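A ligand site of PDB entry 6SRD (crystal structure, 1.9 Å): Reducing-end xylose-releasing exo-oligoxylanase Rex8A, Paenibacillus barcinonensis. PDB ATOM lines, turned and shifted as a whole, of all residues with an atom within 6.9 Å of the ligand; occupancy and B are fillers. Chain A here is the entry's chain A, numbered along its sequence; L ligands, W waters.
An oxygen (O4) of the ligand sits at hydrogen-bond distance from the side-chain carboxylate of Glu 70.
An oxygen (O1) of the ligand lies within hydrogen-bond range of a ring nitrogen (NE2) of His 321 (2.6 Å).
The guanidinium group of Arg 68 is in hydrogen-bond range of an oxygen (O3) of the ligand (3.0 Å).
An oxygen (O2) of the ligand is in hydrogen-bond range of the side-chain carboxylate (OD2) of Asp 61 (2.6 Å).
OE2 of Glu 242 sits at hydrogen-bond distance from N of Asp 265, at 3.1 Å.
OD1 of Asp 61 is in hydrogen-bond range of N of Gly 63.
O of Ser 264 lies within hydrogen-bond range of OH of Tyr 361.
NH2 of Arg 68 lies close to ND2 of Asn 64, at 3.2 Å.
The side-chain hydroxyl of Thr 62 is in hydrogen-bond range of the backbone NH of Tyr 360.
NE of Arg 68 lies within salt-bridge range of OD2 of Asp 61.
OE1 of Glu 70 is in hydrogen-bond range of OH of Tyr 360, 2.6 Å away.
A ring nitrogen (ND1) of His 321 sits close to the backbone carbonyl oxygen (O) of Arg 358, 3.4 Å away.
Merely in contact with the ligand: Asp 265 (3.5 Å), Tyr 360 (3.6 Å), Ser 264 (3.7 Å), Asn 64 (3.7 Å) and Tyr 361 (3.9 Å).
Hydrophobic or aromatic side chains within 4 Å of the ligand: His 321, Tyr 360 and Tyr 361.
Along chain A the residues within 4 Å of the ligand span positions 61 to 361.
Water W2 lies within hydrogen-bond range of OG of Ser 264 (2.5 Å) and O5 of the ligand (2.7 Å).
Water W1 lies within hydrogen-bond range of OD1 of Asp 61 (2.6 Å), O2 of the ligand (2.8 Å), NH1 of Arg 358 (3.1 Å) and ND2 of Asn 64 (3.4 Å).
Water W3 lies within hydrogen-bond range of an oxygen (O1) of the ligand (2.9 Å), the side-chain amide nitrogen of Asn 64 (3.0 Å) and the guanidinium group of Arg 358 (3.5 Å).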
ATOM      1  N   ASP A  61      -8.215 -13.852   5.458  1.00  0.00           N
ATOM      2  CA  ASP A  61      -9.505 -13.884   6.194  1.00  0.00           C
ATOM      3  C   ASP A  61     -10.397 -14.870   5.438  1.00  0.00           C
ATOM      4  O   ASP A  61     -10.994 -14.514   4.413  1.00  0.00           O
ATOM      5  CB  ASP A  61     -10.160 -12.510   6.384  1.00  0.00           C
ATOM      6  CG  ASP A  61     -11.483 -12.557   7.144  1.00  0.00           C
ATOM      7  OD1 ASP A  61     -12.121 -13.664   7.195  1.00  0.00           O
ATOM      8  OD2 ASP A  61     -11.866 -11.509   7.712  1.00  0.00           O
ATOM      9  N   THR A  62     -10.405 -16.116   5.921  1.00  0.00           N
ATOM     10  CA  THR A  62     -11.073 -17.264   5.263  1.00  0.00           C
ATOM     11  C   THR A  62     -12.576 -16.981   5.157  1.00  0.00           C
ATOM     12  O   THR A  62     -13.185 -17.455   4.177  1.00  0.00           O
ATOM     13  CB  THR A  62     -10.793 -18.553   6.043  1.00  0.00           C
ATOM     14  OG1 THR A  62     -11.236 -18.333   7.376  1.00  0.00           O
ATOM     15  CG2 THR A  62      -9.322 -18.936   6.011  1.00  0.00           C
ATOM     16  N   GLY A  63     -13.144 -16.282   6.139  1.00  0.00           N
ATOM     17  CA  GLY A  63     -14.578 -15.980   6.222  1.00  0.00           C
ATOM     18  C   GLY A  63     -15.015 -14.953   5.196  1.00  0.00           C
ATOM     19  O   GLY A  63     -16.121 -15.100   4.632  1.00  0.00           O
ATOM     20  N   ASN A  64     -14.180 -13.940   4.958  1.00  0.00           N
ATOM     21  CA  ASN A  64     -14.513 -12.765   4.113  1.00  0.00           C
ATOM     22  C   ASN A  64     -13.845 -12.900   2.736  1.00  0.00           C
ATOM     23  O   ASN A  64     -14.161 -12.087   1.862  1.00  0.00           O
ATOM     24  CB  ASN A  64     -14.189 -11.479   4.863  1.00  0.00           C
ATOM     25  CG  ASN A  64     -15.134 -11.258   6.026  1.00  0.00           C
ATOM     26  OD1 ASN A  64     -16.341 -11.095   5.837  1.00  0.00           O
ATOM     27  ND2 ASN A  64     -14.603 -11.241   7.242  1.00  0.00           N
ATOM     28  N   ASP A  66     -10.793 -12.233   1.805  1.00  0.00           N
ATOM     29  CA  ASP A  66      -9.940 -11.063   1.493  1.00  0.00           C
ATOM     30  C   ASP A  66      -8.717 -11.102   2.397  1.00  0.00           C
ATOM     31  O   ASP A  66      -8.607 -12.026   3.251  1.00  0.00           O
ATOM     32  CB  ASP A  66     -10.738  -9.756   1.581  1.00  0.00           C
ATOM     33  CG  ASP A  66     -11.304  -9.453   2.963  1.00  0.00           C
ATOM     34  OD1 ASP A  66     -10.905 -10.126   3.940  1.00  0.00           O
ATOM     35  OD2 ASP A  66     -12.125  -8.527   3.060  1.00  0.00           O
ATOM     36  N   ARG A  68      -6.507  -8.746   4.997  1.00  0.00           N
ATOM     37  CA  ARG A  68      -6.782  -7.571   5.856  1.00  0.00           C
ATOM     38  C   ARG A  68      -5.466  -7.107   6.477  1.00  0.00           C
ATOM     39  O   ARG A  68      -4.612  -7.972   6.773  1.00  0.00           O
ATOM     40  CB  ARG A  68      -7.825  -7.980   6.894  1.00  0.00           C
ATOM     41  CG  ARG A  68      -9.184  -8.258   6.275  1.00  0.00           C
ATOM     42  CD  ARG A  68     -10.253  -8.800   7.213  1.00  0.00           C
ATOM     43  NE  ARG A  68     -11.460  -8.802   6.399  1.00  0.00           N
ATOM     44  CZ  ARG A  68     -12.685  -8.542   6.813  1.00  0.00           C
ATOM     45  NH1 ARG A  68     -12.923  -8.296   8.101  1.00  0.00           N
ATOM     46  NH2 ARG A  68     -13.666  -8.508   5.935  1.00  0.00           N
ATOM     47  N   GLU A  70      -5.174  -6.095   9.396  1.00  0.00           N
ATOM     48  CA  GLU A  70      -5.255  -6.866  10.667  1.00  0.00           C
ATOM     49  C   GLU A  70      -4.453  -8.180  10.559  1.00  0.00           C
ATOM     50  O   GLU A  70      -3.526  -8.391  11.377  1.00  0.00           O
ATOM     51  CB  GLU A  70      -6.732  -7.108  10.984  1.00  0.00           C
ATOM     52  CG  GLU A  70      -6.987  -8.035  12.151  1.00  0.00           C
ATOM     53  CD  GLU A  70      -8.424  -8.544  12.144  1.00  0.00           C
ATOM     54  OE1 GLU A  70      -8.767  -9.267  11.195  1.00  0.00           O
ATOM     55  OE2 GLU A  70      -9.207  -8.180  13.075  1.00  0.00           O
ATOM     56  N   GLY A  71      -4.816  -9.058   9.619  1.00  0.00           N
ATOM     57  CA  GLY A  71      -4.248 -10.417   9.506  1.00  0.00           C
ATOM     58  C   GLY A  71      -2.795 -10.382   9.062  1.00  0.00           C
ATOM     59  O   GLY A  71      -1.993 -11.165   9.537  1.00  0.00           O
ATOM     60  N   TYR A  74      -0.840  -9.230  12.091  1.00  0.00           N
ATOM     61  CA  TYR A  74      -0.891 -10.387  13.025  1.00  0.00           C
ATOM     62  C   TYR A  74       0.160 -11.422  12.617  1.00  0.00           C
ATOM     63  O   TYR A  74       0.956 -11.852  13.483  1.00  0.00           O
ATOM     64  CB  TYR A  74      -2.282 -11.030  13.045  1.00  0.00           C
ATOM     65  CG  TYR A  74      -3.310 -10.328  13.898  1.00  0.00           C
ATOM     66  CD1 TYR A  74      -3.010  -9.230  14.688  1.00  0.00           C
ATOM     67  CD2 TYR A  74      -4.607 -10.793  13.913  1.00  0.00           C
ATOM     68  CE1 TYR A  74      -3.981  -8.624  15.459  1.00  0.00           C
ATOM     69  CE2 TYR A  74      -5.596 -10.198  14.671  1.00  0.00           C
ATOM     70  CZ  TYR A  74      -5.280  -9.115  15.459  1.00  0.00           C
ATOM     71  OH  TYR A  74      -6.262  -8.518  16.194  1.00  0.00           O
ATOM     72  N   TRP A 112      -7.076  -1.194   4.291  1.00  0.00           N
ATOM     73  CA  TRP A 112      -7.411  -2.145   5.381  1.00  0.00           C
ATOM     74  C   TRP A 112      -7.672  -3.537   4.797  1.00  0.00           C
ATOM     75  O   TRP A 112      -7.502  -4.534   5.543  1.00  0.00           O
ATOM     76  CB  TRP A 112      -8.562  -1.645   6.242  1.00  0.00           C
ATOM     77  CG  TRP A 112      -9.933  -1.758   5.652  1.00  0.00           C
ATOM     78  CD1 TRP A 112     -10.605  -0.801   4.949  1.00  0.00           C
ATOM     79  CD2 TRP A 112     -10.859  -2.858   5.810  1.00  0.00           C
ATOM     80  NE1 TRP A 112     -11.870  -1.223   4.645  1.00  0.00           N
ATOM     81  CE2 TRP A 112     -12.053  -2.489   5.152  1.00  0.00           C
ATOM     82  CE3 TRP A 112     -10.781  -4.114   6.408  1.00  0.00           C
ATOM     83  CZ2 TRP A 112     -13.158  -3.339   5.081  1.00  0.00           C
ATOM     84  CZ3 TRP A 112     -11.878  -4.951   6.352  1.00  0.00           C
ATOM     85  CH2 TRP A 112     -13.048  -4.570   5.685  1.00  0.00           C
ATOM     86  N   ASP A 128      -5.550  -0.636  14.033  1.00  0.00           N
ATOM     87  CA  ASP A 128      -5.000  -1.825  14.752  1.00  0.00           C
ATOM     88  C   ASP A 128      -3.974  -2.531  13.848  1.00  0.00           C
ATOM     89  O   ASP A 128      -3.054  -3.207  14.391  1.00  0.00           O
ATOM     90  CB  ASP A 128      -6.104  -2.771  15.237  1.00  0.00           C
ATOM     91  CG  ASP A 128      -7.018  -3.335  14.145  1.00  0.00           C
ATOM     92  OD1 ASP A 128      -7.286  -2.610  13.138  1.00  0.00           O
ATOM     93  OD2 ASP A 128      -7.486  -4.502  14.330  1.00  0.00           O
ATOM     94  N   TYR A 197      -8.499  -1.930  20.156  1.00  0.00           N
ATOM     95  CA  TYR A 197      -7.345  -1.286  19.448  1.00  0.00           C
ATOM     96  C   TYR A 197      -6.321  -0.726  20.455  1.00  0.00           C
ATOM     97  O   TYR A 197      -5.226  -0.345  19.995  1.00  0.00           O
ATOM     98  CB  TYR A 197      -7.829  -0.174  18.513  1.00  0.00           C
ATOM     99  CG  TYR A 197      -8.611  -0.557  17.285  1.00  0.00           C
ATOM    100  CD1 TYR A 197      -9.099  -1.828  17.052  1.00  0.00           C
ATOM    101  CD2 TYR A 197      -8.909   0.413  16.339  1.00  0.00           C
ATOM    102  CE1 TYR A 197      -9.826  -2.129  15.895  1.00  0.00           C
ATOM    103  CE2 TYR A 197      -9.623   0.144  15.192  1.00  0.00           C
ATOM    104  CZ  TYR A 197     -10.092  -1.141  14.967  1.00  0.00           C
ATOM    105  OH  TYR A 197     -10.824  -1.403  13.825  1.00  0.00           O
ATOM    106  N   GLU A 242     -17.678  -3.236  21.275  1.00  0.00           N
ATOM    107  CA  GLU A 242     -16.772  -3.256  20.099  1.00  0.00           C
ATOM    108  C   GLU A 242     -16.316  -1.823  19.782  1.00  0.00           C
ATOM    109  O   GLU A 242     -15.107  -1.623  19.640  1.00  0.00           O
ATOM    110  CB  GLU A 242     -17.427  -3.991  18.936  1.00  0.00           C
ATOM    111  CG  GLU A 242     -17.554  -5.479  19.168  1.00  0.00           C
ATOM    112  CD  GLU A 242     -18.051  -6.185  17.930  1.00  0.00           C
ATOM    113  OE1 GLU A 242     -19.272  -6.029  17.640  1.00  0.00           O
ATOM    114  OE2 GLU A 242     -17.220  -6.789  17.210  1.00  0.00           O
ATOM    115  N   TYR A 263     -18.815  -8.674  21.267  1.00  0.00           N
ATOM    116  CA  TYR A 263     -18.697  -9.509  20.035  1.00  0.00           C
ATOM    117  C   TYR A 263     -17.239  -9.455  19.585  1.00  0.00           C
ATOM    118  O   TYR A 263     -16.386  -8.926  20.308  1.00  0.00           O
ATOM    119  CB  TYR A 263     -19.692  -9.031  18.972  1.00  0.00           C
ATOM    120  CG  TYR A 263     -20.171 -10.115  18.029  1.00  0.00           C
ATOM    121  CD1 TYR A 263     -20.882 -11.198  18.503  1.00  0.00           C
ATOM    122  CD2 TYR A 263     -19.945 -10.036  16.660  1.00  0.00           C
ATOM    123  CE1 TYR A 263     -21.353 -12.191  17.654  1.00  0.00           C
ATOM    124  CE2 TYR A 263     -20.413 -11.013  15.796  1.00  0.00           C
ATOM    125  CZ  TYR A 263     -21.118 -12.098  16.301  1.00  0.00           C
ATOM    126  OH  TYR A 263     -21.580 -13.078  15.468  1.00  0.00           O
ATOM    127  N   SER A 264     -16.966 -10.004  18.400  1.00  0.00           N
ATOM    128  CA  SER A 264     -15.624 -10.341  17.851  1.00  0.00           C
ATOM    129  C   SER A 264     -14.492  -9.380  18.262  1.00  0.00           C
ATOM    130  O   SER A 264     -13.523  -9.861  18.917  1.00  0.00           O
ATOM    131  CB  SER A 264     -15.764 -10.457  16.359  1.00  0.00           C
ATOM    132  OG  SER A 264     -16.704 -11.485  16.044  1.00  0.00           O
ATOM    133  N   ASP A 265     -14.532  -8.095  17.892  1.00  0.00           N
ATOM    134  CA  ASP A 265     -13.448  -7.118  18.208  1.00  0.00           C
ATOM    135  C   ASP A 265     -13.084  -7.139  19.707  1.00  0.00           C
ATOM    136  O   ASP A 265     -11.889  -7.274  20.043  1.00  0.00           O
ATOM    137  CB  ASP A 265     -13.842  -5.687  17.814  1.00  0.00           C
ATOM    138  CG  ASP A 265     -13.621  -5.345  16.343  1.00  0.00           C
ATOM    139  OD1 ASP A 265     -13.727  -6.256  15.494  1.00  0.00           O
ATOM    140  OD2 ASP A 265     -13.349  -4.153  16.061  1.00  0.00           O
ATOM    141  N   ARG A 268     -10.499  -9.189  22.206  1.00  0.00           N
ATOM    142  CA  ARG A 268      -9.028  -8.921  22.313  1.00  0.00           C
ATOM    143  C   ARG A 268      -8.734  -8.058  23.554  1.00  0.00           C
ATOM    144  O   ARG A 268      -7.574  -8.058  24.008  1.00  0.00           O
ATOM    145  CB  ARG A 268      -8.499  -8.306  21.018  1.00  0.00           C
ATOM    146  CG  ARG A 268      -8.674  -9.215  19.804  1.00  0.00           C
ATOM    147  CD  ARG A 268      -8.422  -8.541  18.483  1.00  0.00           C
ATOM    148  NE  ARG A 268      -9.400  -7.485  18.201  1.00  0.00           N
ATOM    149  CZ  ARG A 268      -9.537  -6.870  17.031  1.00  0.00           C
ATOM    150  NH1 ARG A 268      -8.795  -7.231  16.004  1.00  0.00           N
ATOM    151  NH2 ARG A 268     -10.447  -5.921  16.882  1.00  0.00           N
ATOM    152  N   LEU A 320     -19.689 -15.688  16.636  1.00  0.00           N
ATOM    153  CA  LEU A 320     -19.176 -16.119  15.320  1.00  0.00           C
ATOM    154  C   LEU A 320     -17.831 -16.825  15.529  1.00  0.00           C
ATOM    155  O   LEU A 320     -17.552 -17.795  14.803  1.00  0.00           O
ATOM    156  CB  LEU A 320     -19.026 -14.890  14.425  1.00  0.00           C
ATOM    157  CG  LEU A 320     -18.691 -15.146  12.951  1.00  0.00           C
ATOM    158  CD1 LEU A 320     -19.720 -16.062  12.295  1.00  0.00           C
ATOM    159  CD2 LEU A 320     -18.611 -13.816  12.214  1.00  0.00           C
ATOM    160  N   HIS A 321     -17.041 -16.351  16.498  1.00  0.00           N
ATOM    161  CA  HIS A 321     -15.657 -16.824  16.758  1.00  0.00           C
ATOM    162  C   HIS A 321     -15.524 -17.285  18.204  1.00  0.00           C
ATOM    163  O   HIS A 321     -14.850 -16.636  19.007  1.00  0.00           O
ATOM    164  CB  HIS A 321     -14.640 -15.732  16.383  1.00  0.00           C
ATOM    165  CG  HIS A 321     -14.752 -15.315  14.952  1.00  0.00           C
ATOM    166  ND1 HIS A 321     -14.433 -16.166  13.919  1.00  0.00           N
ATOM    167  CD2 HIS A 321     -15.160 -14.160  14.391  1.00  0.00           C
ATOM    168  CE1 HIS A 321     -14.651 -15.553  12.774  1.00  0.00           C
ATOM    169  NE2 HIS A 321     -15.089 -14.315  13.036  1.00  0.00           N
ATOM    170  N   ARG A 358     -14.655 -20.245   8.779  1.00  0.00           N
ATOM    171  CA  ARG A 358     -14.621 -19.137   9.775  1.00  0.00           C
ATOM    172  C   ARG A 358     -13.331 -19.162  10.613  1.00  0.00           C
ATOM    173  O   ARG A 358     -13.261 -18.419  11.618  1.00  0.00           O
ATOM    174  CB  ARG A 358     -15.904 -19.214  10.616  1.00  0.00           C
ATOM    175  CG  ARG A 358     -17.113 -18.640   9.905  1.00  0.00           C
ATOM    176  CD  ARG A 358     -16.876 -17.163   9.600  1.00  0.00           C
ATOM    177  NE  ARG A 358     -17.867 -16.566   8.712  1.00  0.00           N
ATOM    178  CZ  ARG A 358     -17.835 -15.312   8.274  1.00  0.00           C
ATOM    179  NH1 ARG A 358     -16.846 -14.504   8.625  1.00  0.00           N
ATOM    180  NH2 ARG A 358     -18.782 -14.886   7.465  1.00  0.00           N
ATOM    181  N   TYR A 360     -10.145 -18.138  10.415  1.00  0.00           N
ATOM    182  CA  TYR A 360      -9.057 -17.110  10.418  1.00  0.00           C
ATOM    183  C   TYR A 360      -8.975 -16.399  11.780  1.00  0.00           C
ATOM    184  O   TYR A 360      -7.928 -16.477  12.435  1.00  0.00           O
ATOM    185  CB  TYR A 360      -9.233 -16.122   9.259  1.00  0.00           C
ATOM    186  CG  TYR A 360      -8.660 -14.743   9.464  1.00  0.00           C
ATOM    187  CD1 TYR A 360      -7.318 -14.468   9.266  1.00  0.00           C
ATOM    188  CD2 TYR A 360      -9.482 -13.680   9.786  1.00  0.00           C
ATOM    189  CE1 TYR A 360      -6.805 -13.190   9.405  1.00  0.00           C
ATOM    190  CE2 TYR A 360      -8.994 -12.383   9.929  1.00  0.00           C
ATOM    191  CZ  TYR A 360      -7.644 -12.145   9.726  1.00  0.00           C
ATOM    192  OH  TYR A 360      -7.167 -10.878   9.867  1.00  0.00           O
ATOM    193  N   TYR A 361     -10.054 -15.731  12.206  1.00  0.00           N
ATOM    194  CA  TYR A 361     -10.028 -14.876  13.423  1.00  0.00           C
ATOM    195  C   TYR A 361      -9.790 -15.720  14.680  1.00  0.00           C
ATOM    196  O   TYR A 361      -8.954 -15.358  15.543  1.00  0.00           O
ATOM    197  CB  TYR A 361     -11.300 -14.047  13.496  1.00  0.00           C
ATOM    198  CG  TYR A 361     -11.227 -12.940  14.523  1.00  0.00           C
ATOM    199  CD1 TYR A 361     -10.332 -11.887  14.396  1.00  0.00           C
ATOM    200  CD2 TYR A 361     -12.082 -12.940  15.613  1.00  0.00           C
ATOM    201  CE1 TYR A 361     -10.286 -10.865  15.334  1.00  0.00           C
ATOM    202  CE2 TYR A 361     -12.033 -11.947  16.567  1.00  0.00           C
ATOM    203  CZ  TYR A 361     -11.124 -10.912  16.430  1.00  0.00           C
ATOM    204  OH  TYR A 361     -11.125  -9.945  17.394  1.00  0.00           O
HETATM  205  O1  LIG L   1     -15.002 -12.244  11.485  1.00  0.00           O
HETATM  206  C1  LIG L   1     -14.023 -11.428  12.126  1.00  0.00           C
HETATM  207  C2  LIG L   1     -13.150 -10.793  11.033  1.00  0.00           C
HETATM  208  C3  LIG L   1     -12.096  -9.871  11.595  1.00  0.00           C
HETATM  209  C4  LIG L   1     -12.794  -8.824  12.461  1.00  0.00           C
HETATM  210  C5  LIG L   1     -13.714  -9.515  13.473  1.00  0.00           C
HETATM  211  O2  LIG L   1     -12.560 -11.819  10.237  1.00  0.00           O
HETATM  212  O3  LIG L   1     -11.381  -9.237  10.528  1.00  0.00           O
HETATM  213  O4  LIG L   1     -11.811  -8.028  13.148  1.00  0.00           O
HETATM  214  O5  LIG L   1     -14.667 -10.387  12.849  1.00  0.00           O
HETATM  215  O   HOH W   1     -13.864 -14.030   9.118  1.00  0.00           O
HETATM  216  O   HOH W   2     -17.244 -10.629  13.731  1.00  0.00           O
HETATM  217  O   HOH W   3     -16.689 -11.124   9.391  1.00  0.00           O
